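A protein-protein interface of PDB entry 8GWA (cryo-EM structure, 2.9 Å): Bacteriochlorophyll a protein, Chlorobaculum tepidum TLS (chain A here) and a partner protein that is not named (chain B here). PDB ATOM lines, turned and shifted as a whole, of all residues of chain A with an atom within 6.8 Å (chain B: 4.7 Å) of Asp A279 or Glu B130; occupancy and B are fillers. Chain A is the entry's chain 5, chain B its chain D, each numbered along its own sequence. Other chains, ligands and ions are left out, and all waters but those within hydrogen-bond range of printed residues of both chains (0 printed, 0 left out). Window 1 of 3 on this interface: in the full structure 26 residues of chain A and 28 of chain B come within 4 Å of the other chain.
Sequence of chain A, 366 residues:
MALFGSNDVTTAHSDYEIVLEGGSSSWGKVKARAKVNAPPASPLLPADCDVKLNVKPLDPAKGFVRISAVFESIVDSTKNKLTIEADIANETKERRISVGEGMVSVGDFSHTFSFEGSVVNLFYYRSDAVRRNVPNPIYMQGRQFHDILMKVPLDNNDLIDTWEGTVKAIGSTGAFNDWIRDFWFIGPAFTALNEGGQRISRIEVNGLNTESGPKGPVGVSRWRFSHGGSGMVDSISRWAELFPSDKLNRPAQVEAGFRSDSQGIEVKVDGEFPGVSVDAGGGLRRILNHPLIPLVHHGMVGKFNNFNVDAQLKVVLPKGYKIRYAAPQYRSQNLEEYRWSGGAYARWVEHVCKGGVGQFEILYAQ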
ATOM      1  N   SER A  24       4.892  32.336  -1.500  1.00  0.00           N
ATOM      2  CA  SER A  24       6.117  31.628  -1.842  1.00  0.00           C
ATOM      3  C   SER A  24       7.064  31.491  -0.658  1.00  0.00           C
ATOM      4  O   SER A  24       8.006  30.694  -0.732  1.00  0.00           O
ATOM      5  CB  SER A  24       6.833  32.341  -2.991  1.00  0.00           C
ATOM      6  OG  SER A  24       6.907  33.736  -2.756  1.00  0.00           O
ATOM      7  N   SER A  26       8.684  30.353   2.845  1.00  0.00           N
ATOM      8  CA  SER A  26       8.748  29.072   3.539  1.00  0.00           C
ATOM      9  C   SER A  26       9.227  29.253   4.972  1.00  0.00           C
ATOM     10  O   SER A  26       9.659  28.294   5.615  1.00  0.00           O
ATOM     11  CB  SER A  26       9.663  28.099   2.803  1.00  0.00           C
ATOM     12  OG  SER A  26      11.017  28.366   3.116  1.00  0.00           O
ATOM     13  N   LYS A 247      16.066  30.611  -0.746  1.00  0.00           N
ATOM     14  CA  LYS A 247      14.882  31.166  -0.102  1.00  0.00           C
ATOM     15  C   LYS A 247      15.208  31.766   1.265  1.00  0.00           C
ATOM     16  O   LYS A 247      14.428  31.671   2.214  1.00  0.00           O
ATOM     17  CB  LYS A 247      13.785  30.105  -0.033  1.00  0.00           C
ATOM     18  CG  LYS A 247      14.101  28.887   0.808  1.00  0.00           C
ATOM     19  CD  LYS A 247      12.952  27.897   0.730  1.00  0.00           C
ATOM     20  CE  LYS A 247      13.211  26.665   1.575  1.00  0.00           C
ATOM     21  NZ  LYS A 247      14.335  25.865   1.019  1.00  0.00           N
ATOM     22  N   SER A 277       8.486  24.903   6.093  1.00  0.00           N
ATOM     23  CA  SER A 277       7.481  24.311   5.223  1.00  0.00           C
ATOM     24  C   SER A 277       8.036  24.213   3.810  1.00  0.00           C
ATOM     25  O   SER A 277       8.432  25.224   3.224  1.00  0.00           O
ATOM     26  CB  SER A 277       6.195  25.135   5.233  1.00  0.00           C
ATOM     27  OG  SER A 277       6.430  26.452   4.771  1.00  0.00           O
ATOM     28  N   VAL A 278       8.063  23.000   3.269  1.00  0.00           N
ATOM     29  CA  VAL A 278       8.545  22.747   1.919  1.00  0.00           C
ATOM     30  C   VAL A 278       7.374  22.283   1.066  1.00  0.00           C
ATOM     31  O   VAL A 278       6.452  21.629   1.563  1.00  0.00           O
ATOM     32  CB  VAL A 278       9.684  21.707   1.902  1.00  0.00           C
ATOM     33  CG1 VAL A 278      10.891  22.236   2.655  1.00  0.00           C
ATOM     34  CG2 VAL A 278       9.216  20.392   2.504  1.00  0.00           C
ATOM     35  N   ASP A 279       7.404  22.645  -0.214  1.00  0.00           N
ATOM     36  CA  ASP A 279       6.368  22.201  -1.135  1.00  0.00           C
ATOM     37  C   ASP A 279       6.406  20.684  -1.256  1.00  0.00           C
ATOM     38  O   ASP A 279       7.423  20.105  -1.647  1.00  0.00           O
ATOM     39  CB  ASP A 279       6.569  22.854  -2.503  1.00  0.00           C
ATOM     40  CG  ASP A 279       5.414  22.604  -3.455  1.00  0.00           C
ATOM     41  OD1 ASP A 279       4.460  21.896  -3.081  1.00  0.00           O
ATOM     42  OD2 ASP A 279       5.460  23.124  -4.590  1.00  0.00           O
ATOM     43  N   ALA A 280       5.292  20.040  -0.916  1.00  0.00           N
ATOM     44  CA  ALA A 280       5.206  18.591  -1.004  1.00  0.00           C
ATOM     45  C   ALA A 280       5.068  18.101  -2.435  1.00  0.00           C
ATOM     46  O   ALA A 280       5.248  16.905  -2.682  1.00  0.00           O
ATOM     47  CB  ALA A 280       4.026  18.077  -0.177  1.00  0.00           C
ATOM     48  N   GLY A 281       4.769  18.991  -3.377  1.00  0.00           N
ATOM     49  CA  GLY A 281       4.593  18.610  -4.761  1.00  0.00           C
ATOM     50  C   GLY A 281       3.283  19.099  -5.338  1.00  0.00           C
ATOM     51  O   GLY A 281       2.213  18.804  -4.803  1.00  0.00           O
ATOM     52  N   GLY A 282       3.355  19.840  -6.438  1.00  0.00           N
ATOM     53  CA  GLY A 282       2.161  20.347  -7.093  1.00  0.00           C
ATOM     54  C   GLY A 282       1.379  21.366  -6.294  1.00  0.00           C
ATOM     55  O   GLY A 282       0.146  21.287  -6.235  1.00  0.00           O
ATOM     56  N   GLY A 283       2.065  22.328  -5.679  1.00  0.00           N
ATOM     57  CA  GLY A 283       1.418  23.376  -4.924  1.00  0.00           C
ATOM     58  C   GLY A 283       1.048  23.009  -3.503  1.00  0.00           C
ATOM     59  O   GLY A 283       0.671  23.896  -2.728  1.00  0.00           O
ATOM     60  N   LEU A 284       1.140  21.733  -3.138  1.00  0.00           N
ATOM     61  CA  LEU A 284       0.803  21.311  -1.788  1.00  0.00           C
ATOM     62  C   LEU A 284       2.004  21.523  -0.879  1.00  0.00           C
ATOM     63  O   LEU A 284       3.040  20.879  -1.054  1.00  0.00           O
ATOM     64  CB  LEU A 284       0.401  19.835  -1.762  1.00  0.00           C
ATOM     65  CG  LEU A 284      -0.906  19.347  -2.394  1.00  0.00           C
ATOM     66  CD1 LEU A 284      -0.795  19.244  -3.910  1.00  0.00           C
ATOM     67  CD2 LEU A 284      -1.324  18.017  -1.798  1.00  0.00           C
ATOM     68  N   ARG A 285       1.869  22.412   0.093  1.00  0.00           N
ATOM     69  CA  ARG A 285       2.931  22.616   1.065  1.00  0.00           C
ATOM     70  C   ARG A 285       2.849  21.557   2.156  1.00  0.00           C
ATOM     71  O   ARG A 285       1.831  20.882   2.327  1.00  0.00           O
ATOM     72  CB  ARG A 285       2.857  24.016   1.679  1.00  0.00           C
ATOM     73  CG  ARG A 285       2.912  25.150   0.673  1.00  0.00           C
ATOM     74  CD  ARG A 285       4.269  25.197  -0.004  1.00  0.00           C
ATOM     75  NE  ARG A 285       5.342  25.442   0.952  1.00  0.00           N
ATOM     76  CZ  ARG A 285       5.741  26.644   1.341  1.00  0.00           C
ATOM     77  NH1 ARG A 285       5.182  27.745   0.866  1.00  0.00           N
ATOM     78  NH2 ARG A 285       6.725  26.745   2.229  1.00  0.00           N
ATOM     79  N   ARG A 286       3.946  21.416   2.894  1.00  0.00           N
ATOM     80  CA  ARG A 286       4.001  20.489   4.011  1.00  0.00           C
ATOM     81  C   ARG A 286       5.088  20.943   4.969  1.00  0.00           C
ATOM     82  O   ARG A 286       6.065  21.577   4.560  1.00  0.00           O
ATOM     83  CB  ARG A 286       4.292  19.047   3.571  1.00  0.00           C
ATOM     84  CG  ARG A 286       5.743  18.809   3.165  1.00  0.00           C
ATOM     85  CD  ARG A 286       6.176  17.362   3.369  1.00  0.00           C
ATOM     86  NE  ARG A 286       5.473  16.413   2.516  1.00  0.00           N
ATOM     87  CZ  ARG A 286       5.970  15.907   1.395  1.00  0.00           C
ATOM     88  NH1 ARG A 286       7.172  16.244   0.957  1.00  0.00           N
ATOM     89  NH2 ARG A 286       5.242  15.041   0.696  1.00  0.00           N
ATOM     90  N   PHE B 120       9.156  33.085  -6.404  1.00  0.00           N
ATOM     91  CA  PHE B 120       9.964  33.980  -5.592  1.00  0.00           C
ATOM     92  C   PHE B 120      11.283  34.271  -6.297  1.00  0.00           C
ATOM     93  O   PHE B 120      11.715  33.533  -7.186  1.00  0.00           O
ATOM     94  CB  PHE B 120      10.221  33.394  -4.196  1.00  0.00           C
ATOM     95  CG  PHE B 120      11.061  32.146  -4.201  1.00  0.00           C
ATOM     96  CD1 PHE B 120      10.504  30.917  -4.516  1.00  0.00           C
ATOM     97  CD2 PHE B 120      12.406  32.202  -3.880  1.00  0.00           C
ATOM     98  CE1 PHE B 120      11.276  29.771  -4.518  1.00  0.00           C
ATOM     99  CE2 PHE B 120      13.181  31.059  -3.879  1.00  0.00           C
ATOM    100  CZ  PHE B 120      12.615  29.843  -4.200  1.00  0.00           C
ATOM    101  N   CYS B 128      12.625  32.084  -9.528  1.00  0.00           N
ATOM    102  CA  CYS B 128      12.717  30.651  -9.306  1.00  0.00           C
ATOM    103  C   CYS B 128      11.516  30.166  -8.509  1.00  0.00           C
ATOM    104  O   CYS B 128      11.073  30.828  -7.566  1.00  0.00           O
ATOM    105  CB  CYS B 128      14.014  30.294  -8.574  1.00  0.00           C
ATOM    106  SG  CYS B 128      14.371  31.325  -7.137  1.00  0.00           S
ATOM    107  N   VAL B 129      10.992  29.005  -8.894  1.00  0.00           N
ATOM    108  CA  VAL B 129       9.825  28.406  -8.259  1.00  0.00           C
ATOM    109  C   VAL B 129      10.256  27.125  -7.555  1.00  0.00           C
ATOM    110  O   VAL B 129      10.956  26.288  -8.138  1.00  0.00           O
ATOM    111  CB  VAL B 129       8.702  28.148  -9.282  1.00  0.00           C
ATOM    112  CG1 VAL B 129       9.156  27.191 -10.371  1.00  0.00           C
ATOM    113  CG2 VAL B 129       7.467  27.610  -8.587  1.00  0.00           C
ATOM    114  N   GLU B 130       9.864  26.990  -6.293  1.00  0.00           N
ATOM    115  CA  GLU B 130      10.201  25.826  -5.481  1.00  0.00           C
ATOM    116  C   GLU B 130       9.028  24.854  -5.513  1.00  0.00           C
ATOM    117  O   GLU B 130       7.963  25.141  -4.956  1.00  0.00           O
ATOM    118  CB  GLU B 130      10.544  26.256  -4.053  1.00  0.00           C
ATOM    119  CG  GLU B 130      11.134  25.170  -3.168  1.00  0.00           C
ATOM    120  CD  GLU B 130      10.080  24.298  -2.528  1.00  0.00           C
ATOM    121  OE1 GLU B 130       8.962  24.802  -2.302  1.00  0.00           O
ATOM    122  OE2 GLU B 130      10.368  23.116  -2.251  1.00  0.00           O
ATOM    123  N   LEU B 131       9.225  23.712  -6.170  1.00  0.00           N
ATOM    124  CA  LEU B 131       8.151  22.755  -6.408  1.00  0.00           C
ATOM    125  C   LEU B 131       8.648  21.344  -6.134  1.00  0.00           C
ATOM    126  O   LEU B 131       9.683  20.934  -6.667  1.00  0.00           O
ATOM    127  CB  LEU B 131       7.627  22.865  -7.846  1.00  0.00           C
ATOM    128  CG  LEU B 131       6.424  22.003  -8.238  1.00  0.00           C
ATOM    129  CD1 LEU B 131       5.486  22.787  -9.133  1.00  0.00           C
ATOM    130  CD2 LEU B 131       6.870  20.728  -8.937  1.00  0.00           C
ATOM    131  N   HIS B 132       7.899  20.612  -5.307  1.00  0.00           N
ATOM    132  CA  HIS B 132       8.203  19.222  -4.961  1.00  0.00           C
ATOM    133  C   HIS B 132       9.595  19.095  -4.344  1.00  0.00           C
ATOM    134  O   HIS B 132      10.425  18.295  -4.782  1.00  0.00           O
ATOM    135  CB  HIS B 132       8.055  18.302  -6.176  1.00  0.00           C
ATOM    136  CG  HIS B 132       7.810  16.869  -5.819  1.00  0.00           C
ATOM    137  ND1 HIS B 132       7.225  15.975  -6.688  1.00  0.00           N
ATOM    138  CD2 HIS B 132       8.063  16.179  -4.682  1.00  0.00           C
ATOM    139  CE1 HIS B 132       7.132  14.794  -6.104  1.00  0.00           C
ATOM    140  NE2 HIS B 132       7.634  14.891  -4.885  1.00  0.00           N
ATOM    141  N   ASN B 133       9.845  19.905  -3.318  1.00  0.00           N
ATOM    142  CA  ASN B 133      11.077  19.904  -2.535  1.00  0.00           C
ATOM    143  C   ASN B 133      12.310  20.222  -3.377  1.00  0.00           C
ATOM    144  O   ASN B 133      13.441  20.036  -2.911  1.00  0.00           O
ATOM    145  CB  ASN B 133      11.266  18.570  -1.799  1.00  0.00           C
ATOM    146  CG  ASN B 133      12.254  18.664  -0.653  1.00  0.00           C
ATOM    147  OD1 ASN B 133      12.671  19.755  -0.265  1.00  0.00           O
ATOM    148  ND2 ASN B 133      12.636  17.516  -0.105  1.00  0.00           N
ATOM    149  N   LYS B 134      12.127  20.699  -4.603  1.00  0.00           N
ATOM    150  CA  LYS B 134      13.231  21.074  -5.470  1.00  0.00           C
ATOM    151  C   LYS B 134      12.980  22.471  -6.021  1.00  0.00           C
ATOM    152  O   LYS B 134      11.853  22.832  -6.367  1.00  0.00           O
ATOM    153  CB  LYS B 134      13.409  20.062  -6.611  1.00  0.00           C
ATOM    154  CG  LYS B 134      14.616  20.315  -7.498  1.00  0.00           C
ATOM    155  CD  LYS B 134      14.769  19.218  -8.537  1.00  0.00           C
ATOM    156  CE  LYS B 134      15.968  19.467  -9.439  1.00  0.00           C
ATOM    157  NZ  LYS B 134      16.119  18.398 -10.465  1.00  0.00           N
ATOM    158  N   ILE B 135      14.050  23.258  -6.104  1.00  0.00           N
ATOM    159  CA  ILE B 135      13.964  24.676  -6.453  1.00  0.00           C
ATOM    160  C   ILE B 135      14.252  24.782  -7.949  1.00  0.00           C
ATOM    161  O   ILE B 135      15.406  24.722  -8.384  1.00  0.00           O
ATOM    162  CB  ILE B 135      14.928  25.544  -5.639  1.00  0.00           C
ATOM    163  CG1 ILE B 135      14.549  25.505  -4.158  1.00  0.00           C
ATOM    164  CG2 ILE B 135      14.914  26.976  -6.147  1.00  0.00           C
ATOM    165  CD1 ILE B 135      15.336  26.462  -3.298  1.00  0.00           C
ATOM    166  N   TYR B 136      13.198  24.933  -8.744  1.00  0.00           N
ATOM    167  CA  TYR B 136      13.328  25.186 -10.169  1.00  0.00           C
ATOM    168  C   TYR B 136      13.421  26.683 -10.430  1.00  0.00           C
ATOM    169  O   TYR B 136      12.934  27.500  -9.646  1.00  0.00           O
ATOM    170  CB  TYR B 136      12.139  24.602 -10.935  1.00  0.00           C
ATOM    171  CG  TYR B 136      12.137  23.095 -11.024  1.00  0.00           C
ATOM    172  CD1 TYR B 136      13.325  22.384 -11.077  1.00  0.00           C
ATOM    173  CD2 TYR B 136      10.946  22.384 -11.047  1.00  0.00           C
ATOM    174  CE1 TYR B 136      13.326  21.008 -11.160  1.00  0.00           C
ATOM    175  CE2 TYR B 136      10.938  21.007 -11.127  1.00  0.00           C
ATOM    176  CZ  TYR B 136      12.131  20.323 -11.183  1.00  0.00           C
ATOM    177  OH  TYR B 136      12.128  18.950 -11.262  1.00  0.00           O
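The side-chain carboxylate (OE1) of Glu B130 sits close to the backbone NH (N) of Asp A279 (3.4 Å).
The backbone carbonyl oxygen of Asp A279 lies within hydrogen-bond range of the backbone NH of Asn B133 (2.9 Å).
OD1 of Asp A279 lies within hydrogen-bond range of N of Gly A281 (2.9 Å).
The side-chain carboxylate of Asp A279 lies close to the backbone NH of Leu A284, at 3.3 Å.
The backbone NH (N) of Cys B128 lies within hydrogen-bond range of the backbone carbonyl oxygen (O) of Phe B120.
The backbone NH (N) of Asn B133 lies close to the side-chain carboxylate (OE2) of Glu B130 (3.4 Å).
Among the printed residues, merely in contact across the chains: Ser A24 with Phe B120, Asp A279 with Leu B131, Asp A279 with His B132, Ala A280 with His B132 and Gly A281 with His B132.
Asp A279 touches just these residues of chain B: Glu B130 (3.1 Å), Leu B131 (3.3 Å), His B132 (3.5 Å) and Asn B133 (2.9 Å).
Of chain A, only Asp A279 (3.1 Å) comes within 4 Å of Glu B130.
Of the printed residues of chain B, Ser A24 touches Phe B120 (3.6 Å).
Printed residues of chain A within 4 Å of Leu B131: Asp A279 (3.3 Å).
Printed residues of chain A within 4 Å of Phe B120: Ser A24 (3.6 Å).
Of the printed residues of chain B, Gly A281 touches His B132.
Tyr B136 touches none of the printed residues of chain A.
The nearest printed residue of chain A that does not touch His B132 is Gly A282 (4.7 Å).
Of the 10 printed residues of chain B, 5 touch a printed residue of chain A.
Printed residues of chain A that touch a printed residue of chain B: Ser A24, Asp A279, Ala A280 and Gly A281.
Along chain A the printed residues that touch a printed residue of chain B span positions 24 to 281.
Among the printed residues, 7 pairs touch across the chains.
Among the printed residues, no Asp or Glu carboxylate lies within 4 Å of a Lys or Arg side-chain nitrogen of the other chain.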
